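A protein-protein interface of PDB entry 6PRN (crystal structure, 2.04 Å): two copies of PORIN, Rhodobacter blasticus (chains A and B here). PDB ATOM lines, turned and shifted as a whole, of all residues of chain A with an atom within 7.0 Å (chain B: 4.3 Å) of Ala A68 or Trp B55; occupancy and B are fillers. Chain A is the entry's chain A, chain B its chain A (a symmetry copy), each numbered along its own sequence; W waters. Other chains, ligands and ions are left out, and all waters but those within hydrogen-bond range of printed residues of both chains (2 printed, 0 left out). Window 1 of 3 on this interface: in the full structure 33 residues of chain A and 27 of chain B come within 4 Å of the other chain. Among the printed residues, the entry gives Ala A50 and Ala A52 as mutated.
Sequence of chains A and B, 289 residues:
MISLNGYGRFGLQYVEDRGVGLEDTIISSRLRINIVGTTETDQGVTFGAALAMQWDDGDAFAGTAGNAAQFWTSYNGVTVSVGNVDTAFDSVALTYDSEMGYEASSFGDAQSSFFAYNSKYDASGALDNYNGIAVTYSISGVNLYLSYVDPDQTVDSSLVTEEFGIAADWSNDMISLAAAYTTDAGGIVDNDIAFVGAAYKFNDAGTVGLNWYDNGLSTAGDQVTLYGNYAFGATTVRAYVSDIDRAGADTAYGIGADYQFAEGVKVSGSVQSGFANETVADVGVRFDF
Water W1 bridges OG of Ser B29 and OD1 of Asn A131.
Water W2 lies within hydrogen-bond range of the backbone carbonyl oxygen (O) of Ala B62, the backbone carbonyl oxygen (O) of Lys A120 and the backbone NH (N) of Ala A68.
The side-chain amide nitrogen (NE2) of Gln B54 sits close to the guanidinium group (NE) of Arg B30 (3.4 Å).
The side-chain amide oxygen of Asn A67 sits at hydrogen-bond distance from the backbone NH of Ala A52 (2.9 Å).
The guanidinium group of Arg B30 lies within salt-bridge range of the side-chain carboxylate of Asp B56, 2.7 Å away.
ND2 of Asn A67 lies within hydrogen-bond range of OH of Tyr A117 (2.9 Å).
The side-chain amide nitrogen of Asn A67 lies close to the side-chain amide nitrogen of Asn A84, 3.4 Å away.
The side-chain amide nitrogen (ND2) of Asn A67 lies within hydrogen-bond range of the backbone carbonyl oxygen (O) of Asn A118 (2.9 Å).
CD1 of Leu A51 touches OG1 of Thr B64, at 3.6 Å.
Gly A66 touches Gly B63.
Ala B62 touches Asn A67.
Gly B63 touches Asn A67 (C to O, 3.996 Å).
Trp B55 touches Ala A68 (NE1 to CB, 3.8 Å).
Ala A69 touches Leu B31 (CB to CD2, 3.8 Å).
Arg B30 touches Phe A71.
CB of Tyr A121 touches CA of Gly B63 (3.8 Å).
Ala B62 touches Leu A127 (CB to CB, 3.5 Å).
Asp A128 touches Asp B59.
The backbone carbonyl oxygen of Asn A67 is in hydrogen-bond range of the side-chain hydroxyl of Thr B64 (2.8 Å).
The backbone carbonyl oxygen (O) of Thr B64 is in hydrogen-bond range of the backbone NH (N) of Gly A66 (2.8 Å).
The backbone NH (N) of Ala A68 sits at hydrogen-bond distance from the backbone carbonyl oxygen (O) of Ala B62, 3.3 Å away.
No position is printed for both chains.
Of the 18 pairs that touch across the chains among the printed residues, none has its exchanged pair printed and touching as well.
Printed residues of chain A that touch a printed residue of chain B: Leu A51, Gly A66, Asn A67, Ala A68, Ala A69, Phe A71, Tyr A121, Leu A127 and Asp A128.
Hydrophobic or aromatic side chains of chain A within 4 Å of the printed part of chain B: Leu A51, Ala A68, Ala A69, Phe A71, Tyr A121 and Leu A127.
Of the 11 printed residues of chain B, 8 touch a printed residue of chain A.
Printed residues of chain B that touch a printed residue of chain A: Ser B29, Arg B30, Leu B31, Trp B55, Asp B59, Ala B62, Gly B63 and Thr B64.
Hydrophobic or aromatic side chains of chain B that line the printed part of chain A: Leu B31, Trp B55 and Ala B62.
Among the printed residues, 18 pairs touch across the chains.
Of the printed residues of chain B, Ala A68 touches Trp B55 and Ala B62.
Of chain A, only Ala A68, Ala A69 and Phe A71 come within 4 Å of Trp B55.
Printed residues of chain B within 4 Å of Asp A128: Asp B59 and Ala B62.
Printed residues of chain B within 4 Å of Leu A127: Ala B62.
Printed residues of chain B within 4 Å of Gly A66: Gly B63 and Thr B64.
Of the printed residues of chain B, Leu A51 touches Thr B64 (3.6 Å).
Gln A70 touches none of the printed residues of chain B.
The nearest printed residue of chain B that does not touch Asp A128 is Asp B57 (4.7 Å).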
ATOM      1  N   ALA A  50     -11.705 -20.291  -1.438  1.00  0.00           N
ATOM      2  CA  ALA A  50     -10.562 -20.861  -0.735  1.00  0.00           C
ATOM      3  C   ALA A  50     -10.895 -21.022   0.766  1.00  0.00           C
ATOM      4  O   ALA A  50     -11.643 -20.245   1.367  1.00  0.00           O
ATOM      5  CB  ALA A  50      -9.348 -19.951  -0.863  1.00  0.00           C
ATOM      6  N   LEU A  51     -10.280 -22.060   1.311  1.00  0.00           N
ATOM      7  CA  LEU A  51     -10.375 -22.411   2.699  1.00  0.00           C
ATOM      8  C   LEU A  51      -8.920 -22.675   3.174  1.00  0.00           C
ATOM      9  O   LEU A  51      -8.144 -23.296   2.417  1.00  0.00           O
ATOM     10  CB  LEU A  51     -11.231 -23.657   2.909  1.00  0.00           C
ATOM     11  CG  LEU A  51     -11.705 -23.938   4.335  1.00  0.00           C
ATOM     12  CD1 LEU A  51     -12.741 -22.873   4.734  1.00  0.00           C
ATOM     13  CD2 LEU A  51     -12.370 -25.328   4.401  1.00  0.00           C
ATOM     14  N   ALA A  52      -8.614 -22.313   4.402  1.00  0.00           N
ATOM     15  CA  ALA A  52      -7.326 -22.689   4.975  1.00  0.00           C
ATOM     16  C   ALA A  52      -7.509 -23.543   6.228  1.00  0.00           C
ATOM     17  O   ALA A  52      -8.437 -23.315   7.045  1.00  0.00           O
ATOM     18  CB  ALA A  52      -6.506 -21.458   5.382  1.00  0.00           C
ATOM     19  N   GLY A  66     -10.961 -25.665   9.672  1.00  0.00           N
ATOM     20  CA  GLY A  66     -10.845 -24.729   8.570  1.00  0.00           C
ATOM     21  C   GLY A  66     -11.288 -23.347   9.126  1.00  0.00           C
ATOM     22  O   GLY A  66     -11.934 -23.282  10.197  1.00  0.00           O
ATOM     23  N   ASN A  67     -10.944 -22.314   8.382  1.00  0.00           N
ATOM     24  CA  ASN A  67     -11.344 -20.955   8.760  1.00  0.00           C
ATOM     25  C   ASN A  67     -12.627 -20.587   7.995  1.00  0.00           C
ATOM     26  O   ASN A  67     -13.326 -21.456   7.471  1.00  0.00           O
ATOM     27  CB  ASN A  67     -10.226 -19.967   8.445  1.00  0.00           C
ATOM     28  CG  ASN A  67      -9.855 -19.913   6.985  1.00  0.00           C
ATOM     29  OD1 ASN A  67     -10.257 -20.784   6.193  1.00  0.00           O
ATOM     30  ND2 ASN A  67      -8.999 -18.978   6.586  1.00  0.00           N
ATOM     31  N   ALA A  68     -12.884 -19.284   7.878  1.00  0.00           N
ATOM     32  CA  ALA A  68     -14.084 -18.868   7.100  1.00  0.00           C
ATOM     33  C   ALA A  68     -13.671 -18.682   5.653  1.00  0.00           C
ATOM     34  O   ALA A  68     -12.527 -18.254   5.370  1.00  0.00           O
ATOM     35  CB  ALA A  68     -14.582 -17.538   7.703  1.00  0.00           C
ATOM     36  N   ALA A  69     -14.571 -18.944   4.735  1.00  0.00           N
ATOM     37  CA  ALA A  69     -14.274 -18.945   3.317  1.00  0.00           C
ATOM     38  C   ALA A  69     -14.048 -17.578   2.718  1.00  0.00           C
ATOM     39  O   ALA A  69     -14.534 -16.565   3.192  1.00  0.00           O
ATOM     40  CB  ALA A  69     -15.535 -19.522   2.541  1.00  0.00           C
ATOM     41  N   GLN A  70     -13.312 -17.600   1.598  1.00  0.00           N
ATOM     42  CA  GLN A  70     -13.060 -16.396   0.822  1.00  0.00           C
ATOM     43  C   GLN A  70     -13.561 -16.759  -0.601  1.00  0.00           C
ATOM     44  O   GLN A  70     -13.282 -17.899  -1.034  1.00  0.00           O
ATOM     45  CB  GLN A  70     -11.552 -16.071   0.721  1.00  0.00           C
ATOM     46  CG  GLN A  70     -11.285 -14.857  -0.182  1.00  0.00           C
ATOM     47  CD  GLN A  70      -9.794 -14.599  -0.312  1.00  0.00           C
ATOM     48  OE1 GLN A  70      -9.238 -14.828  -1.388  1.00  0.00           O
ATOM     49  NE2 GLN A  70      -9.072 -14.277   0.749  1.00  0.00           N
ATOM     50  N   PHE A  71     -14.206 -15.872  -1.305  1.00  0.00           N
ATOM     51  CA  PHE A  71     -14.690 -16.109  -2.647  1.00  0.00           C
ATOM     52  C   PHE A  71     -14.144 -15.010  -3.568  1.00  0.00           C
ATOM     53  O   PHE A  71     -14.015 -13.872  -3.090  1.00  0.00           O
ATOM     54  CB  PHE A  71     -16.223 -16.062  -2.776  1.00  0.00           C
ATOM     55  CG  PHE A  71     -16.914 -16.996  -1.800  1.00  0.00           C
ATOM     56  CD1 PHE A  71     -17.169 -16.554  -0.514  1.00  0.00           C
ATOM     57  CD2 PHE A  71     -17.216 -18.293  -2.155  1.00  0.00           C
ATOM     58  CE1 PHE A  71     -17.759 -17.393   0.439  1.00  0.00           C
ATOM     59  CE2 PHE A  71     -17.840 -19.134  -1.193  1.00  0.00           C
ATOM     60  CZ  PHE A  71     -18.094 -18.688   0.086  1.00  0.00           C
ATOM     61  N   GLY A  83     -16.048 -11.995   1.597  1.00  0.00           N
ATOM     62  CA  GLY A  83     -15.996 -12.874   2.775  1.00  0.00           C
ATOM     63  C   GLY A  83     -14.780 -12.607   3.630  1.00  0.00           C
ATOM     64  O   GLY A  83     -14.574 -11.505   4.124  1.00  0.00           O
ATOM     65  N   ASN A  84     -13.905 -13.626   3.743  1.00  0.00           N
ATOM     66  CA  ASN A  84     -12.681 -13.471   4.565  1.00  0.00           C
ATOM     67  C   ASN A  84     -11.595 -12.977   3.618  1.00  0.00           C
ATOM     68  O   ASN A  84     -10.820 -13.776   3.074  1.00  0.00           O
ATOM     69  CB  ASN A  84     -12.329 -14.857   5.134  1.00  0.00           C
ATOM     70  CG  ASN A  84     -11.158 -14.830   6.121  1.00  0.00           C
ATOM     71  OD1 ASN A  84     -10.586 -13.758   6.444  1.00  0.00           O
ATOM     72  ND2 ASN A  84     -10.777 -16.040   6.561  1.00  0.00           N
ATOM     73  N   VAL A  85     -11.565 -11.676   3.357  1.00  0.00           N
ATOM     74  CA  VAL A  85     -10.680 -11.104   2.352  1.00  0.00           C
ATOM     75  C   VAL A  85      -9.313 -10.692   2.872  1.00  0.00           C
ATOM     76  O   VAL A  85      -9.137 -10.542   4.104  1.00  0.00           O
ATOM     77  CB  VAL A  85     -11.379  -9.877   1.696  1.00  0.00           C
ATOM     78  CG1 VAL A  85     -12.750 -10.314   1.103  1.00  0.00           C
ATOM     79  CG2 VAL A  85     -11.681  -8.765   2.711  1.00  0.00           C
ATOM     80  N   TYR A 117      -6.539 -11.021   6.519  1.00  0.00           N
ATOM     81  CA  TYR A 117      -7.078 -12.363   6.312  1.00  0.00           C
ATOM     82  C   TYR A 117      -7.010 -13.159   7.636  1.00  0.00           C
ATOM     83  O   TYR A 117      -5.967 -13.179   8.261  1.00  0.00           O
ATOM     84  CB  TYR A 117      -6.246 -13.086   5.245  1.00  0.00           C
ATOM     85  CG  TYR A 117      -6.745 -14.474   4.884  1.00  0.00           C
ATOM     86  CD1 TYR A 117      -7.902 -14.672   4.164  1.00  0.00           C
ATOM     87  CD2 TYR A 117      -5.985 -15.582   5.301  1.00  0.00           C
ATOM     88  CE1 TYR A 117      -8.327 -15.983   3.849  1.00  0.00           C
ATOM     89  CE2 TYR A 117      -6.389 -16.891   4.970  1.00  0.00           C
ATOM     90  CZ  TYR A 117      -7.549 -17.058   4.240  1.00  0.00           C
ATOM     91  OH  TYR A 117      -7.970 -18.338   3.945  1.00  0.00           O
ATOM     92  N   ASN A 118      -8.105 -13.790   8.010  1.00  0.00           N
ATOM     93  CA  ASN A 118      -8.122 -14.552   9.289  1.00  0.00           C
ATOM     94  C   ASN A 118      -7.797 -16.027   8.941  1.00  0.00           C
ATOM     95  O   ASN A 118      -8.574 -16.725   8.282  1.00  0.00           O
ATOM     96  CB  ASN A 118      -9.539 -14.503   9.880  1.00  0.00           C
ATOM     97  CG  ASN A 118      -9.932 -13.037  10.204  1.00  0.00           C
ATOM     98  OD1 ASN A 118      -9.173 -12.357  10.884  1.00  0.00           O
ATOM     99  ND2 ASN A 118     -11.075 -12.597   9.699  1.00  0.00           N
ATOM    100  N   SER A 119      -6.633 -16.454   9.367  1.00  0.00           N
ATOM    101  CA  SER A 119      -6.135 -17.801   9.043  1.00  0.00           C
ATOM    102  C   SER A 119      -6.850 -18.921   9.752  1.00  0.00           C
ATOM    103  O   SER A 119      -6.696 -20.095   9.349  1.00  0.00           O
ATOM    104  CB  SER A 119      -4.651 -17.833   9.623  1.00  0.00           C
ATOM    105  OG  SER A 119      -3.765 -17.278   8.662  1.00  0.00           O
ATOM    106  N   LYS A 120      -7.517 -18.647  10.866  1.00  0.00           N
ATOM    107  CA  LYS A 120      -8.132 -19.635  11.699  1.00  0.00           C
ATOM    108  C   LYS A 120      -9.489 -19.211  12.240  1.00  0.00           C
ATOM    109  O   LYS A 120      -9.851 -18.038  12.088  1.00  0.00           O
ATOM    110  CB  LYS A 120      -7.242 -19.727  13.021  1.00  0.00           C
ATOM    111  CG  LYS A 120      -5.844 -20.304  12.707  1.00  0.00           C
ATOM    112  CD  LYS A 120      -5.212 -20.787  14.026  1.00  0.00           C
ATOM    113  CE  LYS A 120      -3.887 -21.467  13.753  1.00  0.00           C
ATOM    114  NZ  LYS A 120      -3.069 -21.539  14.964  1.00  0.00           N
ATOM    115  N   TYR A 121     -10.209 -20.135  12.833  1.00  0.00           N
ATOM    116  CA  TYR A 121     -11.488 -19.876  13.451  1.00  0.00           C
ATOM    117  C   TYR A 121     -11.221 -18.942  14.670  1.00  0.00           C
ATOM    118  O   TYR A 121     -10.039 -18.755  15.050  1.00  0.00           O
ATOM    119  CB  TYR A 121     -12.107 -21.200  13.934  1.00  0.00           C
ATOM    120  CG  TYR A 121     -11.448 -21.792  15.168  1.00  0.00           C
ATOM    121  CD1 TYR A 121     -11.872 -21.467  16.458  1.00  0.00           C
ATOM    122  CD2 TYR A 121     -10.431 -22.703  15.033  1.00  0.00           C
ATOM    123  CE1 TYR A 121     -11.278 -22.026  17.596  1.00  0.00           C
ATOM    124  CE2 TYR A 121      -9.810 -23.278  16.145  1.00  0.00           C
ATOM    125  CZ  TYR A 121     -10.259 -22.939  17.419  1.00  0.00           C
ATOM    126  OH  TYR A 121      -9.620 -23.522  18.493  1.00  0.00           O
ATOM    127  N   LEU A 127     -15.723 -13.076  15.116  1.00  0.00           N
ATOM    128  CA  LEU A 127     -15.739 -13.035  13.652  1.00  0.00           C
ATOM    129  C   LEU A 127     -16.969 -13.657  13.021  1.00  0.00           C
ATOM    130  O   LEU A 127     -16.977 -13.773  11.784  1.00  0.00           O
ATOM    131  CB  LEU A 127     -14.491 -13.795  13.160  1.00  0.00           C
ATOM    132  CG  LEU A 127     -13.137 -13.225  13.595  1.00  0.00           C
ATOM    133  CD1 LEU A 127     -12.011 -14.075  13.009  1.00  0.00           C
ATOM    134  CD2 LEU A 127     -13.018 -11.760  13.146  1.00  0.00           C
ATOM    135  N   ASP A 128     -17.987 -14.037  13.783  1.00  0.00           N
ATOM    136  CA  ASP A 128     -19.081 -14.842  13.212  1.00  0.00           C
ATOM    137  C   ASP A 128     -19.823 -14.168  12.076  1.00  0.00           C
ATOM    138  O   ASP A 128     -20.246 -14.849  11.142  1.00  0.00           O
ATOM    139  CB  ASP A 128     -20.107 -15.264  14.282  1.00  0.00           C
ATOM    140  CG  ASP A 128     -19.566 -16.244  15.313  1.00  0.00           C
ATOM    141  OD1 ASP A 128     -18.353 -16.571  15.397  1.00  0.00           O
ATOM    142  OD2 ASP A 128     -20.393 -16.686  16.118  1.00  0.00           O
ATOM    143  N   TYR A 130     -18.517 -11.452  10.377  1.00  0.00           N
ATOM    144  CA  TYR A 130     -17.529 -10.603   9.750  1.00  0.00           C
ATOM    145  C   TYR A 130     -17.557 -10.885   8.250  1.00  0.00           C
ATOM    146  O   TYR A 130     -17.532 -12.025   7.735  1.00  0.00           O
ATOM    147  CB  TYR A 130     -16.195 -10.842  10.419  1.00  0.00           C
ATOM    148  CG  TYR A 130     -14.908 -10.332   9.813  1.00  0.00           C
ATOM    149  CD1 TYR A 130     -14.452 -10.823   8.588  1.00  0.00           C
ATOM    150  CD2 TYR A 130     -14.161  -9.407  10.541  1.00  0.00           C
ATOM    151  CE1 TYR A 130     -13.219 -10.385   8.092  1.00  0.00           C
ATOM    152  CE2 TYR A 130     -12.928  -8.973  10.049  1.00  0.00           C
ATOM    153  CZ  TYR A 130     -12.455  -9.466   8.827  1.00  0.00           C
ATOM    154  OH  TYR A 130     -11.248  -9.052   8.359  1.00  0.00           O
ATOM    155  N   ASN A 131     -17.622  -9.788   7.485  1.00  0.00           N
ATOM    156  CA  ASN A 131     -17.655  -9.927   6.028  1.00  0.00           C
ATOM    157  C   ASN A 131     -16.944  -8.757   5.381  1.00  0.00           C
ATOM    158  O   ASN A 131     -17.235  -7.588   5.754  1.00  0.00           O
ATOM    159  CB  ASN A 131     -19.113  -9.948   5.529  1.00  0.00           C
ATOM    160  CG  ASN A 131     -19.146 -10.409   4.082  1.00  0.00           C
ATOM    161  OD1 ASN A 131     -18.928 -11.600   3.860  1.00  0.00           O
ATOM    162  ND2 ASN A 131     -19.405  -9.499   3.162  1.00  0.00           N
ATOM    163  N   SER B  29     -23.435 -16.344   1.794  1.00  0.00           N
ATOM    164  CA  SER B  29     -22.529 -17.152   0.951  1.00  0.00           C
ATOM    165  C   SER B  29     -22.305 -18.518   1.575  1.00  0.00           C
ATOM    166  O   SER B  29     -22.599 -18.709   2.768  1.00  0.00           O
ATOM    167  CB  SER B  29     -21.215 -16.386   0.766  1.00  0.00           C
ATOM    168  OG  SER B  29     -20.568 -16.169   1.991  1.00  0.00           O
ATOM    169  N   ARG B  30     -21.862 -19.467   0.735  1.00  0.00           N
ATOM    170  CA  ARG B  30     -21.642 -20.821   1.265  1.00  0.00           C
ATOM    171  C   ARG B  30     -20.483 -21.469   0.479  1.00  0.00           C
ATOM    172  O   ARG B  30     -20.376 -21.295  -0.735  1.00  0.00           O
ATOM    173  CB  ARG B  30     -22.907 -21.662   1.029  1.00  0.00           C
ATOM    174  CG  ARG B  30     -22.670 -23.182   1.258  1.00  0.00           C
ATOM    175  CD  ARG B  30     -23.959 -23.935   0.977  1.00  0.00           C
ATOM    176  NE  ARG B  30     -24.990 -23.668   1.965  1.00  0.00           N
ATOM    177  CZ  ARG B  30     -26.187 -24.279   1.953  1.00  0.00           C
ATOM    178  NH1 ARG B  30     -26.460 -25.176   1.019  1.00  0.00           N
ATOM    179  NH2 ARG B  30     -27.079 -23.990   2.890  1.00  0.00           N
ATOM    180  N   LEU B  31     -19.668 -22.218   1.204  1.00  0.00           N
ATOM    181  CA  LEU B  31     -18.656 -23.013   0.523  1.00  0.00           C
ATOM    182  C   LEU B  31     -18.908 -24.485   0.926  1.00  0.00           C
ATOM    183  O   LEU B  31     -19.087 -24.739   2.152  1.00  0.00           O
ATOM    184  CB  LEU B  31     -17.258 -22.562   0.919  1.00  0.00           C
ATOM    185  CG  LEU B  31     -16.126 -23.539   0.495  1.00  0.00           C
ATOM    186  CD1 LEU B  31     -16.026 -23.607  -1.001  1.00  0.00           C
ATOM    187  CD2 LEU B  31     -14.819 -23.017   1.122  1.00  0.00           C
ATOM    188  N   GLN B  54     -18.629 -27.863   5.132  1.00  0.00           N
ATOM    189  CA  GLN B  54     -19.485 -26.801   4.642  1.00  0.00           C
ATOM    190  C   GLN B  54     -19.435 -25.596   5.574  1.00  0.00           C
ATOM    191  O   GLN B  54     -19.569 -25.729   6.806  1.00  0.00           O
ATOM    192  CB  GLN B  54     -20.943 -27.270   4.515  1.00  0.00           C
ATOM    193  CG  GLN B  54     -21.838 -26.161   3.843  1.00  0.00           C
ATOM    194  CD  GLN B  54     -23.258 -26.728   3.695  1.00  0.00           C
ATOM    195  OE1 GLN B  54     -23.406 -27.777   3.065  1.00  0.00           O
ATOM    196  NE2 GLN B  54     -24.281 -26.090   4.258  1.00  0.00           N
ATOM    197  N   TRP B  55     -19.250 -24.430   4.951  1.00  0.00           N
ATOM    198  CA  TRP B  55     -19.227 -23.192   5.747  1.00  0.00           C
ATOM    199  C   TRP B  55     -20.356 -22.288   5.220  1.00  0.00           C
ATOM    200  O   TRP B  55     -20.527 -22.241   3.980  1.00  0.00           O
ATOM    201  CB  TRP B  55     -17.894 -22.445   5.543  1.00  0.00           C
ATOM    202  CG  TRP B  55     -17.943 -21.077   6.211  1.00  0.00           C
ATOM    203  CD1 TRP B  55     -17.659 -20.796   7.510  1.00  0.00           C
ATOM    204  CD2 TRP B  55     -18.252 -19.813   5.577  1.00  0.00           C
ATOM    205  NE1 TRP B  55     -17.839 -19.463   7.772  1.00  0.00           N
ATOM    206  CE2 TRP B  55     -18.171 -18.830   6.584  1.00  0.00           C
ATOM    207  CE3 TRP B  55     -18.672 -19.448   4.314  1.00  0.00           C
ATOM    208  CZ2 TRP B  55     -18.468 -17.486   6.347  1.00  0.00           C
ATOM    209  CZ3 TRP B  55     -18.936 -18.095   4.044  1.00  0.00           C
ATOM    210  CH2 TRP B  55     -18.838 -17.141   5.078  1.00  0.00           C
ATOM    211  N   ASP B  56     -21.062 -21.643   6.100  1.00  0.00           N
ATOM    212  CA  ASP B  56     -22.102 -20.667   5.710  1.00  0.00           C
ATOM    213  C   ASP B  56     -21.872 -19.363   6.452  1.00  0.00           C
ATOM    214  O   ASP B  56     -21.397 -19.365   7.591  1.00  0.00           O
ATOM    215  CB  ASP B  56     -23.526 -21.175   6.104  1.00  0.00           C
ATOM    216  CG  ASP B  56     -23.979 -22.269   5.138  1.00  0.00           C
ATOM    217  OD1 ASP B  56     -24.575 -21.994   4.092  1.00  0.00           O
ATOM    218  OD2 ASP B  56     -23.776 -23.454   5.481  1.00  0.00           O
ATOM    219  N   ASP B  57     -22.278 -18.236   5.842  1.00  0.00           N
ATOM    220  CA  ASP B  57     -22.070 -16.953   6.539  1.00  0.00           C
ATOM    221  C   ASP B  57     -22.815 -16.996   7.867  1.00  0.00           C
ATOM    222  O   ASP B  57     -23.887 -17.623   7.944  1.00  0.00           O
ATOM    223  CB  ASP B  57     -22.567 -15.776   5.653  1.00  0.00           C
ATOM    224  CG  ASP B  57     -24.019 -15.902   5.342  1.00  0.00           C
ATOM    225  OD1 ASP B  57     -24.410 -16.587   4.384  1.00  0.00           O
ATOM    226  OD2 ASP B  57     -24.870 -15.322   6.074  1.00  0.00           O
ATOM    227  N   ASP B  59     -21.845 -18.689  10.477  1.00  0.00           N
ATOM    228  CA  ASP B  59     -21.542 -19.886  11.255  1.00  0.00           C
ATOM    229  C   ASP B  59     -20.724 -19.522  12.506  1.00  0.00           C
ATOM    230  O   ASP B  59     -19.790 -18.711  12.523  1.00  0.00           O
ATOM    231  CB  ASP B  59     -20.719 -20.958  10.493  1.00  0.00           C
ATOM    232  CG  ASP B  59     -21.565 -21.857   9.633  1.00  0.00           C
ATOM    233  OD1 ASP B  59     -22.789 -21.804   9.700  1.00  0.00           O
ATOM    234  OD2 ASP B  59     -20.959 -22.616   8.820  1.00  0.00           O
ATOM    235  N   ALA B  62     -16.613 -18.746  13.153  1.00  0.00           N
ATOM    236  CA  ALA B  62     -16.001 -18.404  11.893  1.00  0.00           C
ATOM    237  C   ALA B  62     -15.024 -19.498  11.445  1.00  0.00           C
ATOM    238  O   ALA B  62     -13.892 -19.252  11.010  1.00  0.00           O
ATOM    239  CB  ALA B  62     -15.318 -17.031  11.987  1.00  0.00           C
ATOM    240  N   GLY B  63     -15.476 -20.735  11.583  1.00  0.00           N
ATOM    241  CA  GLY B  63     -14.649 -21.896  11.243  1.00  0.00           C
ATOM    242  C   GLY B  63     -15.484 -22.939  10.489  1.00  0.00           C
ATOM    243  O   GLY B  63     -16.724 -22.818  10.347  1.00  0.00           O
ATOM    244  N   THR B  64     -14.781 -23.949  10.010  1.00  0.00           N
ATOM    245  CA  THR B  64     -15.412 -24.993   9.201  1.00  0.00           C
ATOM    246  C   THR B  64     -14.878 -26.353   9.683  1.00  0.00           C
ATOM    247  O   THR B  64     -13.647 -26.480   9.905  1.00  0.00           O
ATOM    248  CB  THR B  64     -14.944 -24.820   7.714  1.00  0.00           C
ATOM    249  OG1 THR B  64     -15.251 -23.474   7.311  1.00  0.00           O
ATOM    250  CG2 THR B  64     -15.681 -25.783   6.765  1.00  0.00           C
HETATM  251  O   HOH W   1     -20.966 -13.709   3.107  1.00  0.00           O
HETATM  252  O   HOH W   2     -12.025 -17.401  10.167  1.00  0.00           O
